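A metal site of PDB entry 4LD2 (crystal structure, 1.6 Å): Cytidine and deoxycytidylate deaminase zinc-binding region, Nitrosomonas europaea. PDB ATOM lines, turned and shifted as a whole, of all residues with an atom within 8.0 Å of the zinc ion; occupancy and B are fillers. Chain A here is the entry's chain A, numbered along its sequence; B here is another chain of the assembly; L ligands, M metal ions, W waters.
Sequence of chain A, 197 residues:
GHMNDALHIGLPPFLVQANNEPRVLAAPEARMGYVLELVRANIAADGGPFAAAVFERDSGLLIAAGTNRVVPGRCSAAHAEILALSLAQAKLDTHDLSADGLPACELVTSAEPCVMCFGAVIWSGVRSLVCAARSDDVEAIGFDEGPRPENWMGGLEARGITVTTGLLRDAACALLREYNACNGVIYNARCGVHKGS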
ATOM      1  N   PHE A  50     -25.143  -4.735  16.525  1.00  0.00           N
ATOM      2  CA  PHE A  50     -26.484  -4.776  15.976  1.00  0.00           C
ATOM      3  C   PHE A  50     -26.701  -5.985  15.085  1.00  0.00           C
ATOM      4  O   PHE A  50     -25.810  -6.369  14.313  1.00  0.00           O
ATOM      5  CB  PHE A  50     -26.747  -3.505  15.159  1.00  0.00           C
ATOM      6  CG  PHE A  50     -26.640  -2.239  15.955  1.00  0.00           C
ATOM      7  CD1 PHE A  50     -27.714  -1.799  16.721  1.00  0.00           C
ATOM      8  CD2 PHE A  50     -25.451  -1.526  15.978  1.00  0.00           C
ATOM      9  CE1 PHE A  50     -27.598  -0.653  17.504  1.00  0.00           C
ATOM     10  CE2 PHE A  50     -25.325  -0.375  16.753  1.00  0.00           C
ATOM     11  CZ  PHE A  50     -26.409   0.065  17.519  1.00  0.00           C
ATOM     12  N   ASN A  68     -24.406  -5.718  11.655  1.00  0.00           N
ATOM     13  CA  ASN A  68     -23.706  -4.500  11.267  1.00  0.00           C
ATOM     14  C   ASN A  68     -22.285  -4.867  10.851  1.00  0.00           C
ATOM     15  O   ASN A  68     -21.508  -5.368  11.664  1.00  0.00           O
ATOM     16  CB  ASN A  68     -23.693  -3.500  12.426  1.00  0.00           C
ATOM     17  CG  ASN A  68     -22.960  -2.224  12.084  1.00  0.00           C
ATOM     18  OD1 ASN A  68     -21.784  -2.248  11.736  1.00  0.00           O
ATOM     19  ND2 ASN A  68     -23.647  -1.094  12.183  1.00  0.00           N
ATOM     20  N   VAL A  70     -20.427  -2.508   8.964  1.00  0.00           N
ATOM     21  CA  VAL A  70     -19.936  -1.229   8.456  1.00  0.00           C
ATOM     22  C   VAL A  70     -18.415  -1.100   8.401  1.00  0.00           C
ATOM     23  O   VAL A  70     -17.853  -0.798   7.350  1.00  0.00           O
ATOM     24  CB  VAL A  70     -20.506  -0.054   9.278  1.00  0.00           C
ATOM     25  CG1 VAL A  70     -19.870   1.263   8.830  1.00  0.00           C
ATOM     26  CG2 VAL A  70     -22.016   0.006   9.108  1.00  0.00           C
ATOM     27  N   SER A  76     -20.740   2.077   4.878  1.00  0.00           N
ATOM     28  CA  SER A  76     -21.617   2.697   5.867  1.00  0.00           C
ATOM     29  C   SER A  76     -23.081   2.261   5.781  1.00  0.00           C
ATOM     30  O   SER A  76     -23.827   2.410   6.743  1.00  0.00           O
ATOM     31  CB  SER A  76     -21.517   4.229   5.800  1.00  0.00           C
ATOM     32  OG  SER A  76     -21.900   4.756   4.548  1.00  0.00           O
ATOM     33  N   ALA A  77     -23.474   1.716   4.635  1.00  0.00           N
ATOM     34  CA  ALA A  77     -24.851   1.260   4.457  1.00  0.00           C
ATOM     35  C   ALA A  77     -25.042  -0.166   4.966  1.00  0.00           C
ATOM     36  O   ALA A  77     -26.169  -0.659   5.015  1.00  0.00           O
ATOM     37  CB  ALA A  77     -25.244   1.332   2.987  1.00  0.00           C
ATOM     38  N   ALA A  78     -23.951  -0.814   5.364  1.00  0.00           N
ATOM     39  CA  ALA A  78     -24.023  -2.199   5.841  1.00  0.00           C
ATOM     40  C   ALA A  78     -24.583  -2.384   7.250  1.00  0.00           C
ATOM     41  O   ALA A  78     -23.958  -3.031   8.089  1.00  0.00           O
ATOM     42  CB  ALA A  78     -22.652  -2.853   5.733  1.00  0.00           C
ATOM     43  N   HIS A  79     -25.756  -1.820   7.507  1.00  0.00           N
ATOM     44  CA  HIS A  79     -26.382  -1.984   8.809  1.00  0.00           C
ATOM     45  C   HIS A  79     -27.073  -3.339   8.853  1.00  0.00           C
ATOM     46  O   HIS A  79     -27.370  -3.924   7.813  1.00  0.00           O
ATOM     47  CB  HIS A  79     -27.407  -0.881   9.059  1.00  0.00           C
ATOM     48  CG  HIS A  79     -26.784   0.447   9.370  1.00  0.00           C
ATOM     49  ND1 HIS A  79     -27.475   1.469   9.995  1.00  0.00           N
ATOM     50  CD2 HIS A  79     -25.537   0.918   9.160  1.00  0.00           C
ATOM     51  CE1 HIS A  79     -26.685   2.513  10.144  1.00  0.00           C
ATOM     52  NE2 HIS A  79     -25.494   2.203   9.653  1.00  0.00           N
ATOM     53  N   ALA A  80     -27.321  -3.836  10.051  1.00  0.00           N
ATOM     54  CA  ALA A  80     -27.962  -5.135  10.208  1.00  0.00           C
ATOM     55  C   ALA A  80     -29.253  -5.270   9.409  1.00  0.00           C
ATOM     56  O   ALA A  80     -29.464  -6.280   8.737  1.00  0.00           O
ATOM     57  CB  ALA A  80     -28.231  -5.390  11.685  1.00  0.00           C
ATOM     58  N   GLU A  81     -30.092  -4.254   9.461  1.00  0.00           N
ATOM     59  CA  GLU A  81     -31.375  -4.282   8.759  1.00  0.00           C
ATOM     60  C   GLU A  81     -31.203  -4.372   7.241  1.00  0.00           C
ATOM     61  O   GLU A  81     -31.902  -5.132   6.577  1.00  0.00           O
ATOM     62  CB  GLU A  81     -32.204  -3.051   9.121  1.00  0.00           C
ATOM     63  CG  GLU A  81     -32.469  -2.903  10.625  1.00  0.00           C
ATOM     64  CD  GLU A  81     -31.450  -2.014  11.336  1.00  0.00           C
ATOM     65  OE1 GLU A  81     -30.244  -2.284  11.239  1.00  0.00           O
ATOM     66  OE2 GLU A  81     -31.878  -1.039  11.986  1.00  0.00           O
ATOM     67  N   ILE A  82     -30.279  -3.584   6.712  1.00  0.00           N
ATOM     68  CA  ILE A  82     -30.027  -3.584   5.271  1.00  0.00           C
ATOM     69  C   ILE A  82     -29.594  -4.969   4.811  1.00  0.00           C
ATOM     70  O   ILE A  82     -30.077  -5.488   3.805  1.00  0.00           O
ATOM     71  CB  ILE A  82     -28.935  -2.557   4.896  1.00  0.00           C
ATOM     72  CG1 ILE A  82     -29.376  -1.155   5.308  1.00  0.00           C
ATOM     73  CG2 ILE A  82     -28.677  -2.602   3.394  1.00  0.00           C
ATOM     74  CD1 ILE A  82     -30.662  -0.698   4.668  1.00  0.00           C
ATOM     75  N   THR A 109     -35.343  -6.918  14.907  1.00  0.00           N
ATOM     76  CA  THR A 109     -34.090  -6.208  15.045  1.00  0.00           C
ATOM     77  C   THR A 109     -33.687  -5.951  16.510  1.00  0.00           C
ATOM     78  O   THR A 109     -34.540  -5.767  17.374  1.00  0.00           O
ATOM     79  CB  THR A 109     -34.189  -4.879  14.276  1.00  0.00           C
ATOM     80  OG1 THR A 109     -32.928  -4.197  14.305  1.00  0.00           O
ATOM     81  CG2 THR A 109     -35.262  -3.994  14.896  1.00  0.00           C
ATOM     82  N   ALA A 111     -32.364  -3.380  17.811  1.00  0.00           N
ATOM     83  CA  ALA A 111     -32.604  -2.012  18.254  1.00  0.00           C
ATOM     84  C   ALA A 111     -33.474  -1.298  17.239  1.00  0.00           C
ATOM     85  O   ALA A 111     -33.515  -1.679  16.069  1.00  0.00           O
ATOM     86  CB  ALA A 111     -31.273  -1.274  18.398  1.00  0.00           C
ATOM     87  N   GLU A 112     -34.185  -0.262  17.676  1.00  0.00           N
ATOM     88  CA  GLU A 112     -35.032   0.493  16.755  1.00  0.00           C
ATOM     89  C   GLU A 112     -34.118   1.014  15.643  1.00  0.00           C
ATOM     90  O   GLU A 112     -33.006   1.457  15.900  1.00  0.00           O
ATOM     91  CB  GLU A 112     -35.746   1.632  17.495  1.00  0.00           C
ATOM     92  CG  GLU A 112     -36.621   1.102  18.627  1.00  0.00           C
ATOM     93  CD  GLU A 112     -37.448   2.170  19.311  1.00  0.00           C
ATOM     94  OE1 GLU A 112     -37.095   3.365  19.226  1.00  0.00           O
ATOM     95  OE2 GLU A 112     -38.445   1.801  19.966  1.00  0.00           O
ATOM     96  N   PRO A 113     -34.585   0.943  14.389  1.00  0.00           N
ATOM     97  CA  PRO A 113     -33.813   1.383  13.215  1.00  0.00           C
ATOM     98  C   PRO A 113     -33.447   2.854  13.117  1.00  0.00           C
ATOM     99  O   PRO A 113     -34.179   3.735  13.579  1.00  0.00           O
ATOM    100  CB  PRO A 113     -34.694   0.937  12.058  1.00  0.00           C
ATOM    101  CG  PRO A 113     -36.080   1.115  12.607  1.00  0.00           C
ATOM    102  CD  PRO A 113     -35.941   0.510  13.994  1.00  0.00           C
ATOM    103  N   CYS A 114     -32.295   3.118  12.508  1.00  0.00           N
ATOM    104  CA  CYS A 114     -31.835   4.481  12.291  1.00  0.00           C
ATOM    105  C   CYS A 114     -32.683   4.981  11.130  1.00  0.00           C
ATOM    106  O   CYS A 114     -33.445   4.217  10.543  1.00  0.00           O
ATOM    107  CB  CYS A 114     -30.349   4.493  11.913  1.00  0.00           C
ATOM    108  SG  CYS A 114     -29.997   3.918  10.221  1.00  0.00           S
ATOM    109  N   VAL A 115     -32.541   6.255  10.774  1.00  0.00           N
ATOM    110  CA  VAL A 115     -33.355   6.798   9.685  1.00  0.00           C
ATOM    111  C   VAL A 115     -33.185   6.073   8.341  1.00  0.00           C
ATOM    112  O   VAL A 115     -34.146   5.903   7.598  1.00  0.00           O
ATOM    113  CB  VAL A 115     -33.118   8.315   9.507  1.00  0.00           C
ATOM    114  CG1 VAL A 115     -31.655   8.602   9.229  1.00  0.00           C
ATOM    115  CG2 VAL A 115     -34.000   8.846   8.386  1.00  0.00           C
ATOM    116  N   MET A 116     -31.957   5.651   8.029  1.00  0.00           N
ATOM    117  CA  MET A 116     -31.701   4.939   6.777  1.00  0.00           C
ATOM    118  C   MET A 116     -32.440   3.595   6.755  1.00  0.00           C
ATOM    119  O   MET A 116     -33.107   3.265   5.775  1.00  0.00           O
ATOM    120  CB  MET A 116     -30.201   4.698   6.598  1.00  0.00           C
ATOM    121  CG  MET A 116     -29.858   3.804   5.415  1.00  0.00           C
ATOM    122  SD  MET A 116     -28.085   3.497   5.273  1.00  0.00           S
ATOM    123  CE  MET A 116     -27.819   2.418   6.699  1.00  0.00           C
ATOM    124  N   CYS A 117     -32.333   2.832   7.830  1.00  0.00           N
ATOM    125  CA  CYS A 117     -32.989   1.534   7.883  1.00  0.00           C
ATOM    126  C   CYS A 117     -34.499   1.647   8.021  1.00  0.00           C
ATOM    127  O   CYS A 117     -35.233   0.749   7.611  1.00  0.00           O
ATOM    128  CB  CYS A 117     -32.390   0.701   9.019  1.00  0.00           C
ATOM    129  SG  CYS A 117     -30.652   0.326   8.687  1.00  0.00           S
ATOM    130  N   PHE A 118     -34.941   2.760   8.590  1.00  0.00           N
ATOM    131  CA  PHE A 118     -36.371   3.045   8.726  1.00  0.00           C
ATOM    132  C   PHE A 118     -36.915   3.096   7.287  1.00  0.00           C
ATOM    133  O   PHE A 118     -37.933   2.474   6.974  1.00  0.00           O
ATOM    134  CB  PHE A 118     -36.534   4.402   9.418  1.00  0.00           C
ATOM    135  CG  PHE A 118     -37.887   5.035   9.226  1.00  0.00           C
ATOM    136  CD1 PHE A 118     -39.014   4.516   9.838  1.00  0.00           C
ATOM    137  CD2 PHE A 118     -38.014   6.183   8.444  1.00  0.00           C
ATOM    138  CE1 PHE A 118     -40.256   5.132   9.673  1.00  0.00           C
ATOM    139  CE2 PHE A 118     -39.237   6.800   8.280  1.00  0.00           C
ATOM    140  CZ  PHE A 118     -40.363   6.281   8.892  1.00  0.00           C
ATOM    141  N   GLY A 119     -36.218   3.819   6.414  1.00  0.00           N
ATOM    142  CA  GLY A 119     -36.657   3.905   5.032  1.00  0.00           C
ATOM    143  C   GLY A 119     -36.545   2.548   4.350  1.00  0.00           C
ATOM    144  O   GLY A 119     -37.430   2.150   3.591  1.00  0.00           O
ATOM    145  N   ALA A 120     -35.462   1.825   4.634  1.00  0.00           N
ATOM    146  CA  ALA A 120     -35.267   0.509   4.036  1.00  0.00           C
ATOM    147  C   ALA A 120     -36.413  -0.445   4.395  1.00  0.00           C
ATOM    148  O   ALA A 120     -36.828  -1.249   3.572  1.00  0.00           O
ATOM    149  CB  ALA A 120     -33.941  -0.087   4.480  1.00  0.00           C
ATOM    150  N   ASP A 144     -26.210   7.089  17.335  1.00  0.00           N
ATOM    151  CA  ASP A 144     -27.107   8.060  16.713  1.00  0.00           C
ATOM    152  C   ASP A 144     -28.097   7.417  15.740  1.00  0.00           C
ATOM    153  O   ASP A 144     -27.699   6.685  14.826  1.00  0.00           O
ATOM    154  CB  ASP A 144     -26.269   9.123  15.994  1.00  0.00           C
ATOM    155  CG  ASP A 144     -27.123  10.145  15.252  1.00  0.00           C
ATOM    156  OD1 ASP A 144     -28.136  10.603  15.798  1.00  0.00           O
ATOM    157  OD2 ASP A 144     -26.749  10.490  14.118  1.00  0.00           O
ATOM    158  N   GLU A 145     -29.379   7.684  15.950  1.00  0.00           N
ATOM    159  CA  GLU A 145     -30.432   7.132  15.110  1.00  0.00           C
ATOM    160  C   GLU A 145     -30.669   8.021  13.898  1.00  0.00           C
ATOM    161  O   GLU A 145     -31.322   7.609  12.940  1.00  0.00           O
ATOM    162  CB  GLU A 145     -31.722   6.991  15.904  1.00  0.00           C
ATOM    163  CG  GLU A 145     -31.646   5.998  17.051  1.00  0.00           C
ATOM    164  CD  GLU A 145     -31.730   4.553  16.569  1.00  0.00           C
ATOM    165  OE1 GLU A 145     -30.992   4.186  15.642  1.00  0.00           O
ATOM    166  OE2 GLU A 145     -32.538   3.788  17.137  1.00  0.00           O
ATOM    167  N   TRP B 123     -24.758   9.156   6.976  1.00  0.00           N
ATOM    168  CA  TRP B 123     -23.757   8.223   7.507  1.00  0.00           C
ATOM    169  C   TRP B 123     -22.531   8.048   6.609  1.00  0.00           C
ATOM    170  O   TRP B 123     -21.495   7.570   7.082  1.00  0.00           O
ATOM    171  CB  TRP B 123     -24.366   6.837   7.719  1.00  0.00           C
ATOM    172  CG  TRP B 123     -25.632   6.793   8.511  1.00  0.00           C
ATOM    173  CD1 TRP B 123     -26.713   5.996   8.269  1.00  0.00           C
ATOM    174  CD2 TRP B 123     -25.936   7.546   9.683  1.00  0.00           C
ATOM    175  NE1 TRP B 123     -27.684   6.207   9.227  1.00  0.00           N
ATOM    176  CE2 TRP B 123     -27.230   7.158  10.102  1.00  0.00           C
ATOM    177  CE3 TRP B 123     -25.244   8.516  10.423  1.00  0.00           C
ATOM    178  CZ2 TRP B 123     -27.849   7.710  11.231  1.00  0.00           C
ATOM    179  CZ3 TRP B 123     -25.863   9.059  11.547  1.00  0.00           C
ATOM    180  CH2 TRP B 123     -27.145   8.651  11.942  1.00  0.00           C
HETATM  181  O1  LIG L   1     -24.372   5.253  16.121  1.00  0.00           O
HETATM  182  C1  LIG L   1     -23.058   5.051  15.823  1.00  0.00           C
HETATM  183  C2  LIG L   1     -22.865   3.721  14.927  1.00  0.00           C
HETATM  184  O2  LIG L   1     -23.500   2.468  15.447  1.00  0.00           O
HETATM  185  C3  LIG L   1     -24.365   1.981  14.244  1.00  0.00           C
HETATM  186  N1  LIG L   1     -25.809   1.995  14.384  1.00  0.00           N
HETATM  187  C4  LIG L   1     -26.446   2.902  15.256  1.00  0.00           C
HETATM  188  C5  LIG L   1     -27.848   2.839  15.457  1.00  0.00           C
HETATM  189  C6  LIG L   1     -28.544   1.882  14.794  1.00  0.00           C
HETATM  190  N2  LIG L   1     -27.857   0.983  13.915  1.00  0.00           N
HETATM  191  C7  LIG L   1     -26.556   1.044  13.723  1.00  0.00           C
HETATM  192  O3  LIG L   1     -26.016   0.194  12.916  1.00  0.00           O
HETATM  193  N3  LIG L   1     -30.013   1.767  14.974  1.00  0.00           N
HETATM  194  C8  LIG L   1     -23.767   2.579  12.949  1.00  0.00           C
HETATM  195  O4  LIG L   1     -22.689   1.786  12.511  1.00  0.00           O
HETATM  196  C9  LIG L   1     -23.370   3.916  13.526  1.00  0.00           C
HETATM  197  O5  LIG L   1     -22.394   4.474  12.702  1.00  0.00           O
HETATM  198 ZN    ZN M   1     -29.562   1.598  10.212  1.00  0.00          ZN
HETATM  199  O   HOH W   1     -30.171   0.884  12.167  1.00  0.00           O
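OE1 of Glu 145 lies within hydrogen-bond range of N3 of the ligand, 2.7 Å away.
A nitrogen (N3) of the ligand is in hydrogen-bond range of the backbone carbonyl oxygen (O) of Glu 112.
The side-chain amide nitrogen (ND2) of Asn 68 is in hydrogen-bond range of an oxygen (O3) of the ligand, at 2.8 Å.
The backbone NH of Asp 144 sits at hydrogen-bond distance from an oxygen (O1) of the ligand.
The backbone carbonyl oxygen (O) of Ser 76 sits close to a ring nitrogen (NE2) of His 79 (3.4 Å).
The side-chain sulfur (SG) of Cys 117 sits close to the side-chain carboxylate (OE1) of Glu 81 (3.7 Å).
The side-chain sulfur of Cys 114 sits close to the backbone NH of Met 116, 3.4 Å away.
The indole nitrogen (NE1) of Trp 123 of chain B sits close to the side-chain sulfur (SG) of Cys 114 (3.4 Å).
Glu 81 touches the zinc ion.
Of the 24 residues printed, 4 come within 4 Å of the zinc ion.
Along chain A the residues within 4 Å of the zinc ion span positions 79 to 117.
The nearest printed residue that does not touch the zinc ion is Met 116 (4.01 Å).
ND1 of His 79 is bound to the zinc ion (2.1 Å).
Water W1 binds the zinc ion, at 2.2 Å.
The zinc ion is bound by the side-chain sulfur (SG) of Cys 117.
The zinc ion is bound by the side-chain sulfur (SG) of Cys 114 (2.4 Å).
Water W1 lies within hydrogen-bond range of OE2 of Glu 81 (2.6 Å), N2 of the ligand (2.9 Å) and N of Cys 114 (3.1 Å).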
